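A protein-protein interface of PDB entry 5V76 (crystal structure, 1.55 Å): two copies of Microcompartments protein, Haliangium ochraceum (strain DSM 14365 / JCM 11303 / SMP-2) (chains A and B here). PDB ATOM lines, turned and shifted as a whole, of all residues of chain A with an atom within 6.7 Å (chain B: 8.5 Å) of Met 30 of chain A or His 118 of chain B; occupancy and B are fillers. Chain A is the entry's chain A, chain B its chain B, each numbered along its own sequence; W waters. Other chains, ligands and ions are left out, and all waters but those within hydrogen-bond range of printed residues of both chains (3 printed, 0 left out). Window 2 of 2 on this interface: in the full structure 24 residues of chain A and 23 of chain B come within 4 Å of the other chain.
OE1 of Gln 21 of chain A is in hydrogen-bond range of ND2 of Asn 124 of chain B, at 3.4 Å. The backbone carbonyl oxygen of Gln 21 of chain A sits at hydrogen-bond distance from the guanidinium group of Arg 125 of chain B (3.0 Å). NE2 of Gln 121 of chain B sits at hydrogen-bond distance from SD of Met 28 of chain A (3.3 Å). The side-chain carboxylate (OE2) of Glu 31 of chain A lies within hydrogen-bond range of the backbone NH (N) of Ala 134 of chain B, at 3.0 Å.
No position is printed for both chains. Of the 9 pairs that touch across the chains among the printed residues, none has its exchanged pair printed and touching as well.
Among the printed residues, pairs that only touch across the chains: Gln 21 of chain A with Gln 121 of chain B (3.4 Å), Met 28 of chain A with Arg 125 of chain B (3.9 Å), Met 30 of chain A with Gly 117 of chain B (3.7 Å), Met 30 of chain A with His 118 of chain B (3.9 Å) and Glu 31 of chain A with Gln 133 of chain B (3.6 Å).
Water W1 lies within hydrogen-bond range of O of Ala 134 of chain B (2.7 Å) and OE1 of Glu 31 of chain A (2.7 Å). Water W3 lies within hydrogen-bond range of OE1 of Gln 21 of chain A (2.7 Å), OG of Ser 120 of chain B (2.9 Å) and ND2 of Asn 124 of chain B (3.3 Å). Water W2 lies within hydrogen-bond range of the backbone carbonyl oxygen of Gly 117 of chain B, the side-chain amide nitrogen of Gln 21 of chain A and the side-chain hydroxyl of Ser 120 of chain B.
The side-chain amide nitrogen (NE2) of Gln 21 of chain A sits at hydrogen-bond distance from the backbone carbonyl oxygen (O) of Pro 29 of chain A, 2.9 Å away. The backbone NH of Met 30 of chain A is in hydrogen-bond range of the side-chain amide oxygen of Gln 33 of chain A. The side-chain carboxylate (OD1) of Asp 116 of chain B sits at hydrogen-bond distance from the backbone NH (N) of His 118 of chain B (2.8 Å). The backbone carbonyl oxygen (O) of Gly 117 of chain B lies within hydrogen-bond range of the side-chain hydroxyl (OG) of Ser 120 of chain B. O of Ser 120 of chain B lies within hydrogen-bond range of ND2 of Asn 124 of chain B (3.1 Å).
Hydrophobic or aromatic side chains of chain B that line the printed part of chain A: His 118 and Ala 134. Among the printed residues, 9 pairs touch across the chains. Among the printed residues, no Asp or Glu carboxylate lies within 4 Å of a Lys or Arg side-chain nitrogen of the other chain.
Of the printed residues of chain B, Gln 21 of chain A touches Gln 121 (3.4 Å), Asn 124 (3.4 Å) and Arg 125 (3.0 Å). Of the printed residues of chain B, Met 28 of chain A touches Gln 121 and Arg 125. Met 30 of chain A touches two residues of chain B. Ile 115 of chain B touches none of the printed residues of chain A. Of chain A, only Met 30 (3.9 Å) comes within 4 Å of His 118 of chain B. Of the printed residues of chain A, Gln 121 of chain B touches Gln 21 (3.4 Å) and Met 28 (3.3 Å). Printed residues of chain A within 4 Å of Asn 124 of chain B: Gln 21 (3.4 Å). Printed residues of chain A within 4 Å of Gln 133 of chain B: Glu 31. The nearest residue of chain A that does not touch His 118 of chain B is Gln 21 of chain A (6.3 Å).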
ATOM      1  N   LEU A  12     -22.435 -21.244  25.221  1.00  0.00           N
ATOM      2  CA  LEU A  12     -21.682 -20.716  24.088  1.00  0.00           C
ATOM      3  C   LEU A  12     -21.827 -21.589  22.844  1.00  0.00           C
ATOM      4  O   LEU A  12     -21.532 -22.792  22.858  1.00  0.00           O
ATOM      5  CB  LEU A  12     -20.204 -20.600  24.460  1.00  0.00           C
ATOM      6  CG  LEU A  12     -19.869 -19.567  25.524  1.00  0.00           C
ATOM      7  CD1 LEU A  12     -18.405 -19.718  25.935  1.00  0.00           C
ATOM      8  CD2 LEU A  12     -20.151 -18.150  25.049  1.00  0.00           C
ATOM      9  N   GLN A  13     -22.201 -20.951  21.734  1.00  0.00           N
ATOM     10  CA  GLN A  13     -22.397 -21.635  20.472  1.00  0.00           C
ATOM     11  C   GLN A  13     -21.064 -21.823  19.751  1.00  0.00           C
ATOM     12  O   GLN A  13     -20.100 -21.087  19.996  1.00  0.00           O
ATOM     13  CB  GLN A  13     -23.381 -20.840  19.617  1.00  0.00           C
ATOM     14  CG  GLN A  13     -24.753 -20.636  20.284  1.00  0.00           C
ATOM     15  CD  GLN A  13     -25.392 -21.957  20.625  1.00  0.00           C
ATOM     16  OE1 GLN A  13     -25.741 -22.743  19.736  1.00  0.00           O
ATOM     17  NE2 GLN A  13     -25.508 -22.236  21.913  1.00  0.00           N
ATOM     18  N   VAL A  17     -17.521 -19.724  20.110  1.00  0.00           N
ATOM     19  CA  VAL A  17     -16.393 -20.366  20.797  1.00  0.00           C
ATOM     20  C   VAL A  17     -15.142 -20.327  19.931  1.00  0.00           C
ATOM     21  O   VAL A  17     -14.046 -20.009  20.415  1.00  0.00           O
ATOM     22  CB  VAL A  17     -16.762 -21.807  21.189  1.00  0.00           C
ATOM     23  CG1 VAL A  17     -15.507 -22.612  21.592  1.00  0.00           C
ATOM     24  CG2 VAL A  17     -17.764 -21.772  22.302  1.00  0.00           C
ATOM     25  N   GLN A  21     -11.758 -18.488  20.936  1.00  0.00           N
ATOM     26  CA  GLN A  21     -10.516 -19.251  20.971  1.00  0.00           C
ATOM     27  C   GLN A  21      -9.433 -18.581  20.160  1.00  0.00           C
ATOM     28  O   GLN A  21      -8.246 -18.793  20.417  1.00  0.00           O
ATOM     29  CB  GLN A  21     -10.747 -20.659  20.448  1.00  0.00           C
ATOM     30  CG  GLN A  21     -11.545 -21.520  21.416  1.00  0.00           C
ATOM     31  CD  GLN A  21     -11.917 -22.873  20.828  1.00  0.00           C
ATOM     32  OE1 GLN A  21     -11.826 -23.088  19.632  1.00  0.00           O
ATOM     33  NE2 GLN A  21     -12.341 -23.793  21.689  1.00  0.00           N
ATOM     34  N   MET A  28      -9.051 -21.067  27.436  1.00  0.00           N
ATOM     35  CA  MET A  28      -9.938 -21.169  26.276  1.00  0.00           C
ATOM     36  C   MET A  28     -11.322 -21.697  26.634  1.00  0.00           C
ATOM     37  O   MET A  28     -11.425 -22.750  27.270  1.00  0.00           O
ATOM     38  CB  MET A  28      -9.302 -22.090  25.273  1.00  0.00           C
ATOM     39  CG  MET A  28      -7.953 -21.619  24.896  1.00  0.00           C
ATOM     40  SD  MET A  28      -8.213 -20.411  23.645  1.00  0.00           S
ATOM     41  CE  MET A  28      -8.544 -18.875  24.260  1.00  0.00           C
ATOM     42  N   PRO A  29     -12.401 -21.054  26.180  1.00  0.00           N
ATOM     43  CA  PRO A  29     -13.734 -21.649  26.326  1.00  0.00           C
ATOM     44  C   PRO A  29     -13.916 -22.812  25.375  1.00  0.00           C
ATOM     45  O   PRO A  29     -13.203 -22.965  24.385  1.00  0.00           O
ATOM     46  CB  PRO A  29     -14.682 -20.501  25.958  1.00  0.00           C
ATOM     47  CG  PRO A  29     -13.916 -19.783  24.910  1.00  0.00           C
ATOM     48  CD  PRO A  29     -12.457 -19.851  25.332  1.00  0.00           C
ATOM     49  N   MET A  30     -14.911 -23.644  25.687  1.00  0.00           N
ATOM     50  CA  MET A  30     -15.271 -24.788  24.863  1.00  0.00           C
ATOM     51  C   MET A  30     -16.764 -24.760  24.539  1.00  0.00           C
ATOM     52  O   MET A  30     -17.558 -24.099  25.206  1.00  0.00           O
ATOM     53  CB  MET A  30     -14.923 -26.103  25.581  1.00  0.00           C
ATOM     54  CG  MET A  30     -13.470 -26.214  25.958  1.00  0.00           C
ATOM     55  SD  MET A  30     -12.407 -26.333  24.517  1.00  0.00           S
ATOM     56  CE  MET A  30     -12.467 -28.079  24.274  1.00  0.00           C
ATOM     57  N   GLU A  31     -17.149 -25.544  23.528  1.00  0.00           N
ATOM     58  CA  GLU A  31     -18.522 -25.526  23.061  1.00  0.00           C
ATOM     59  C   GLU A  31     -19.495 -25.882  24.173  1.00  0.00           C
ATOM     60  O   GLU A  31     -19.270 -26.814  24.954  1.00  0.00           O
ATOM     61  CB  GLU A  31     -18.684 -26.482  21.877  1.00  0.00           C
ATOM     62  CG  GLU A  31     -17.928 -25.961  20.651  1.00  0.00           C
ATOM     63  CD  GLU A  31     -18.009 -26.852  19.432  1.00  0.00           C
ATOM     64  OE1 GLU A  31     -18.877 -27.748  19.402  1.00  0.00           O
ATOM     65  OE2 GLU A  31     -17.192 -26.675  18.505  1.00  0.00           O
ATOM     66  N   GLN A  32     -20.582 -25.123  24.230  1.00  0.00           N
ATOM     67  CA  GLN A  32     -21.716 -25.305  25.135  1.00  0.00           C
ATOM     68  C   GLN A  32     -21.417 -24.915  26.575  1.00  0.00           C
ATOM     69  O   GLN A  32     -22.313 -25.017  27.426  1.00  0.00           O
ATOM     70  CB  GLN A  32     -22.247 -26.749  25.113  1.00  0.00           C
ATOM     71  CG  GLN A  32     -22.610 -27.266  23.720  1.00  0.00           C
ATOM     72  CD  GLN A  32     -23.601 -26.390  22.973  1.00  0.00           C
ATOM     73  OE1 GLN A  32     -24.544 -25.842  23.557  1.00  0.00           O
ATOM     74  NE2 GLN A  32     -23.391 -26.254  21.660  1.00  0.00           N
ATOM     75  N   GLN A  33     -20.226 -24.411  26.883  1.00  0.00           N
ATOM     76  CA  GLN A  33     -19.997 -23.886  28.218  1.00  0.00           C
ATOM     77  C   GLN A  33     -20.836 -22.646  28.444  1.00  0.00           C
ATOM     78  O   GLN A  33     -21.165 -21.921  27.504  1.00  0.00           O
ATOM     79  CB  GLN A  33     -18.520 -23.550  28.420  1.00  0.00           C
ATOM     80  CG  GLN A  33     -17.630 -24.758  28.516  1.00  0.00           C
ATOM     81  CD  GLN A  33     -16.266 -24.407  29.045  1.00  0.00           C
ATOM     82  OE1 GLN A  33     -15.562 -23.597  28.443  1.00  0.00           O
ATOM     83  NE2 GLN A  33     -15.886 -24.986  30.192  1.00  0.00           N
ATOM     84  N   ALA A  34     -21.172 -22.393  29.707  1.00  0.00           N
ATOM     85  CA  ALA A  34     -21.777 -21.129  30.107  1.00  0.00           C
ATOM     86  C   ALA A  34     -20.688 -20.067  30.293  1.00  0.00           C
ATOM     87  O   ALA A  34     -19.523 -20.377  30.531  1.00  0.00           O
ATOM     88  CB  ALA A  34     -22.600 -21.290  31.384  1.00  0.00           C
ATOM     89  N   HIS A  76     -15.963 -18.581  32.301  1.00  0.00           N
ATOM     90  CA  HIS A  76     -16.780 -19.675  31.768  1.00  0.00           C
ATOM     91  C   HIS A  76     -16.592 -20.964  32.570  1.00  0.00           C
ATOM     92  O   HIS A  76     -15.591 -21.170  33.261  1.00  0.00           O
ATOM     93  CB  HIS A  76     -16.459 -19.937  30.298  1.00  0.00           C
ATOM     94  CG  HIS A  76     -15.008 -20.055  30.013  1.00  0.00           C
ATOM     95  ND1 HIS A  76     -14.276 -18.998  29.505  1.00  0.00           N
ATOM     96  CD2 HIS A  76     -14.133 -21.072  30.198  1.00  0.00           C
ATOM     97  CE1 HIS A  76     -13.017 -19.376  29.362  1.00  0.00           C
ATOM     98  NE2 HIS A  76     -12.900 -20.622  29.787  1.00  0.00           N
ATOM     99  N   ASP A  78     -18.396 -25.373  32.506  1.00  0.00           N
ATOM    100  CA  ASP A  78     -19.417 -26.291  32.011  1.00  0.00           C
ATOM    101  C   ASP A  78     -20.770 -26.062  32.672  1.00  0.00           C
ATOM    102  O   ASP A  78     -21.810 -26.312  32.043  1.00  0.00           O
ATOM    103  CB  ASP A  78     -19.015 -27.745  32.261  1.00  0.00           C
ATOM    104  CG  ASP A  78     -17.908 -28.236  31.360  1.00  0.00           C
ATOM    105  OD1 ASP A  78     -17.413 -27.483  30.506  1.00  0.00           O
ATOM    106  OD2 ASP A  78     -17.527 -29.417  31.515  1.00  0.00           O
ATOM    107  N   ILE B 115     -12.445 -34.274  14.837  1.00  0.00           N
ATOM    108  CA  ILE B 115     -11.356 -33.663  15.585  1.00  0.00           C
ATOM    109  C   ILE B 115     -11.831 -33.290  16.983  1.00  0.00           C
ATOM    110  O   ILE B 115     -12.956 -32.822  17.200  1.00  0.00           O
ATOM    111  CB  ILE B 115     -10.742 -32.443  14.875  1.00  0.00           C
ATOM    112  CG1 ILE B 115     -11.758 -31.329  14.668  1.00  0.00           C
ATOM    113  CG2 ILE B 115     -10.038 -32.884  13.579  1.00  0.00           C
ATOM    114  CD1 ILE B 115     -11.077 -30.027  14.294  1.00  0.00           C
ATOM    115  N   ASP B 116     -10.946 -33.508  17.948  1.00  0.00           N
ATOM    116  CA  ASP B 116     -11.185 -33.113  19.317  1.00  0.00           C
ATOM    117  C   ASP B 116     -11.271 -31.588  19.433  1.00  0.00           C
ATOM    118  O   ASP B 116     -10.579 -30.858  18.722  1.00  0.00           O
ATOM    119  CB  ASP B 116     -10.042 -33.666  20.175  1.00  0.00           C
ATOM    120  CG  ASP B 116     -10.247 -33.436  21.642  1.00  0.00           C
ATOM    121  OD1 ASP B 116      -9.868 -32.344  22.117  1.00  0.00           O
ATOM    122  OD2 ASP B 116     -10.803 -34.334  22.326  1.00  0.00           O
ATOM    123  N   GLY B 117     -12.128 -31.117  20.348  1.00  0.00           N
ATOM    124  CA  GLY B 117     -12.290 -29.674  20.546  1.00  0.00           C
ATOM    125  C   GLY B 117     -11.028 -28.950  20.963  1.00  0.00           C
ATOM    126  O   GLY B 117     -10.893 -27.752  20.689  1.00  0.00           O
ATOM    127  N   HIS B 118     -10.076 -29.640  21.586  1.00  0.00           N
ATOM    128  CA  HIS B 118      -8.820 -28.968  21.906  1.00  0.00           C
ATOM    129  C   HIS B 118      -7.970 -28.768  20.659  1.00  0.00           C
ATOM    130  O   HIS B 118      -7.204 -27.799  20.570  1.00  0.00           O
ATOM    131  CB  HIS B 118      -8.028 -29.773  22.943  1.00  0.00           C
ATOM    132  CG  HIS B 118      -8.724 -29.907  24.259  1.00  0.00           C
ATOM    133  ND1 HIS B 118      -9.629 -30.916  24.525  1.00  0.00           N
ATOM    134  CD2 HIS B 118      -8.663 -29.154  25.382  1.00  0.00           C
ATOM    135  CE1 HIS B 118     -10.089 -30.777  25.758  1.00  0.00           C
ATOM    136  NE2 HIS B 118      -9.528 -29.709  26.295  1.00  0.00           N
ATOM    137  N   GLN B 119      -8.072 -29.671  19.687  1.00  0.00           N
ATOM    138  CA  GLN B 119      -7.324 -29.502  18.455  1.00  0.00           C
ATOM    139  C   GLN B 119      -8.001 -28.486  17.539  1.00  0.00           C
ATOM    140  O   GLN B 119      -7.302 -27.760  16.831  1.00  0.00           O
ATOM    141  CB  GLN B 119      -7.142 -30.856  17.736  1.00  0.00           C
ATOM    142  CG  GLN B 119      -6.203 -30.773  16.528  1.00  0.00           C
ATOM    143  CD  GLN B 119      -5.636 -32.127  16.119  1.00  0.00           C
ATOM    144  OE1 GLN B 119      -6.143 -33.150  16.550  1.00  0.00           O
ATOM    145  NE2 GLN B 119      -4.583 -32.133  15.303  1.00  0.00           N
ATOM    146  N   SER B 120      -9.332 -28.386  17.552  1.00  0.00           N
ATOM    147  CA  SER B 120      -9.943 -27.327  16.741  1.00  0.00           C
ATOM    148  C   SER B 120      -9.517 -25.961  17.266  1.00  0.00           C
ATOM    149  O   SER B 120      -9.295 -25.032  16.474  1.00  0.00           O
ATOM    150  CB  SER B 120     -11.468 -27.457  16.677  1.00  0.00           C
ATOM    151  OG  SER B 120     -12.065 -27.459  17.925  1.00  0.00           O
ATOM    152  N   GLN B 121      -9.363 -25.825  18.589  1.00  0.00           N
ATOM    153  CA  GLN B 121      -8.853 -24.572  19.162  1.00  0.00           C
ATOM    154  C   GLN B 121      -7.490 -24.224  18.590  1.00  0.00           C
ATOM    155  O   GLN B 121      -7.255 -23.075  18.180  1.00  0.00           O
ATOM    156  CB  GLN B 121      -8.768 -24.665  20.682  1.00  0.00           C
ATOM    157  CG  GLN B 121      -8.288 -23.385  21.395  1.00  0.00           C
ATOM    158  CD  GLN B 121      -6.796 -23.172  21.347  1.00  0.00           C
ATOM    159  OE1 GLN B 121      -6.006 -24.121  21.334  1.00  0.00           O
ATOM    160  NE2 GLN B 121      -6.393 -21.914  21.314  1.00  0.00           N
ATOM    161  N   LEU B 122      -6.567 -25.202  18.560  1.00  0.00           N
ATOM    162  CA  LEU B 122      -5.221 -24.927  18.070  1.00  0.00           C
ATOM    163  C   LEU B 122      -5.255 -24.447  16.627  1.00  0.00           C
ATOM    164  O   LEU B 122      -4.523 -23.522  16.257  1.00  0.00           O
ATOM    165  CB  LEU B 122      -4.335 -26.166  18.165  1.00  0.00           C
ATOM    166  CG  LEU B 122      -4.004 -26.670  19.572  1.00  0.00           C
ATOM    167  CD1 LEU B 122      -3.506 -28.127  19.451  1.00  0.00           C
ATOM    168  CD2 LEU B 122      -2.975 -25.797  20.248  1.00  0.00           C
ATOM    169  N   ILE B 123      -6.089 -25.079  15.801  1.00  0.00           N
ATOM    170  CA  ILE B 123      -6.206 -24.710  14.389  1.00  0.00           C
ATOM    171  C   ILE B 123      -6.799 -23.308  14.258  1.00  0.00           C
ATOM    172  O   ILE B 123      -6.303 -22.473  13.486  1.00  0.00           O
ATOM    173  CB  ILE B 123      -7.049 -25.760  13.637  1.00  0.00           C
ATOM    174  CG1 ILE B 123      -6.370 -27.142  13.665  1.00  0.00           C
ATOM    175  CG2 ILE B 123      -7.320 -25.334  12.181  1.00  0.00           C
ATOM    176  CD1 ILE B 123      -5.020 -27.224  13.025  1.00  0.00           C
ATOM    177  N   ASN B 124      -7.865 -23.034  15.011  1.00  0.00           N
ATOM    178  CA  ASN B 124      -8.505 -21.719  14.949  1.00  0.00           C
ATOM    179  C   ASN B 124      -7.526 -20.611  15.307  1.00  0.00           C
ATOM    180  O   ASN B 124      -7.540 -19.540  14.696  1.00  0.00           O
ATOM    181  CB  ASN B 124      -9.705 -21.681  15.882  1.00  0.00           C
ATOM    182  CG  ASN B 124     -10.889 -22.418  15.321  1.00  0.00           C
ATOM    183  OD1 ASN B 124     -11.089 -22.407  14.106  1.00  0.00           O
ATOM    184  ND2 ASN B 124     -11.689 -23.042  16.186  1.00  0.00           N
ATOM    185  N   ARG B 125      -6.665 -20.843  16.300  1.00  0.00           N
ATOM    186  CA  ARG B 125      -5.716 -19.813  16.723  1.00  0.00           C
ATOM    187  C   ARG B 125      -4.685 -19.496  15.647  1.00  0.00           C
ATOM    188  O   ARG B 125      -4.253 -18.344  15.524  1.00  0.00           O
ATOM    189  CB  ARG B 125      -5.011 -20.272  17.998  1.00  0.00           C
ATOM    190  CG  ARG B 125      -4.219 -19.188  18.672  1.00  0.00           C
ATOM    191  CD  ARG B 125      -5.125 -18.442  19.620  1.00  0.00           C
ATOM    192  NE  ARG B 125      -4.400 -17.508  20.450  1.00  0.00           N
ATOM    193  CZ  ARG B 125      -4.944 -16.854  21.466  1.00  0.00           C
ATOM    194  NH1 ARG B 125      -6.222 -17.049  21.768  1.00  0.00           N
ATOM    195  NH2 ARG B 125      -4.215 -15.998  22.173  1.00  0.00           N
ATOM    196  N   GLN B 133     -14.833 -26.302  13.770  1.00  0.00           N
ATOM    197  CA  GLN B 133     -15.522 -26.602  15.012  1.00  0.00           C
ATOM    198  C   GLN B 133     -15.248 -28.042  15.426  1.00  0.00           C
ATOM    199  O   GLN B 133     -14.789 -28.864  14.629  1.00  0.00           O
ATOM    200  CB  GLN B 133     -17.026 -26.356  14.894  1.00  0.00           C
ATOM    201  CG  GLN B 133     -17.380 -24.862  14.821  1.00  0.00           C
ATOM    202  CD  GLN B 133     -17.166 -24.261  13.442  1.00  0.00           C
ATOM    203  OE1 GLN B 133     -17.602 -24.827  12.446  1.00  0.00           O
ATOM    204  NE2 GLN B 133     -16.484 -23.107  13.376  1.00  0.00           N
ATOM    205  N   ALA B 134     -15.483 -28.316  16.701  1.00  0.00           N
ATOM    206  CA  ALA B 134     -15.207 -29.642  17.239  1.00  0.00           C
ATOM    207  C   ALA B 134     -16.026 -30.684  16.489  1.00  0.00           C
ATOM    208  O   ALA B 134     -17.189 -30.456  16.162  1.00  0.00           O
ATOM    209  CB  ALA B 134     -15.545 -29.672  18.725  1.00  0.00           C
ATOM    210  N   GLY B 135     -15.400 -31.826  16.223  1.00  0.00           N
ATOM    211  CA  GLY B 135     -16.064 -32.938  15.579  1.00  0.00           C
ATOM    212  C   GLY B 135     -15.999 -32.934  14.074  1.00  0.00           C
ATOM    213  O   GLY B 135     -16.341 -33.948  13.454  1.00  0.00           O
HETATM  214  O   HOH W   1     -19.217 -28.863  16.928  1.00  0.00           O
HETATM  215  O   HOH W   2     -13.319 -26.374  20.649  1.00  0.00           O
HETATM  216  O   HOH W   3     -13.342 -24.910  18.335  1.00  0.00           O
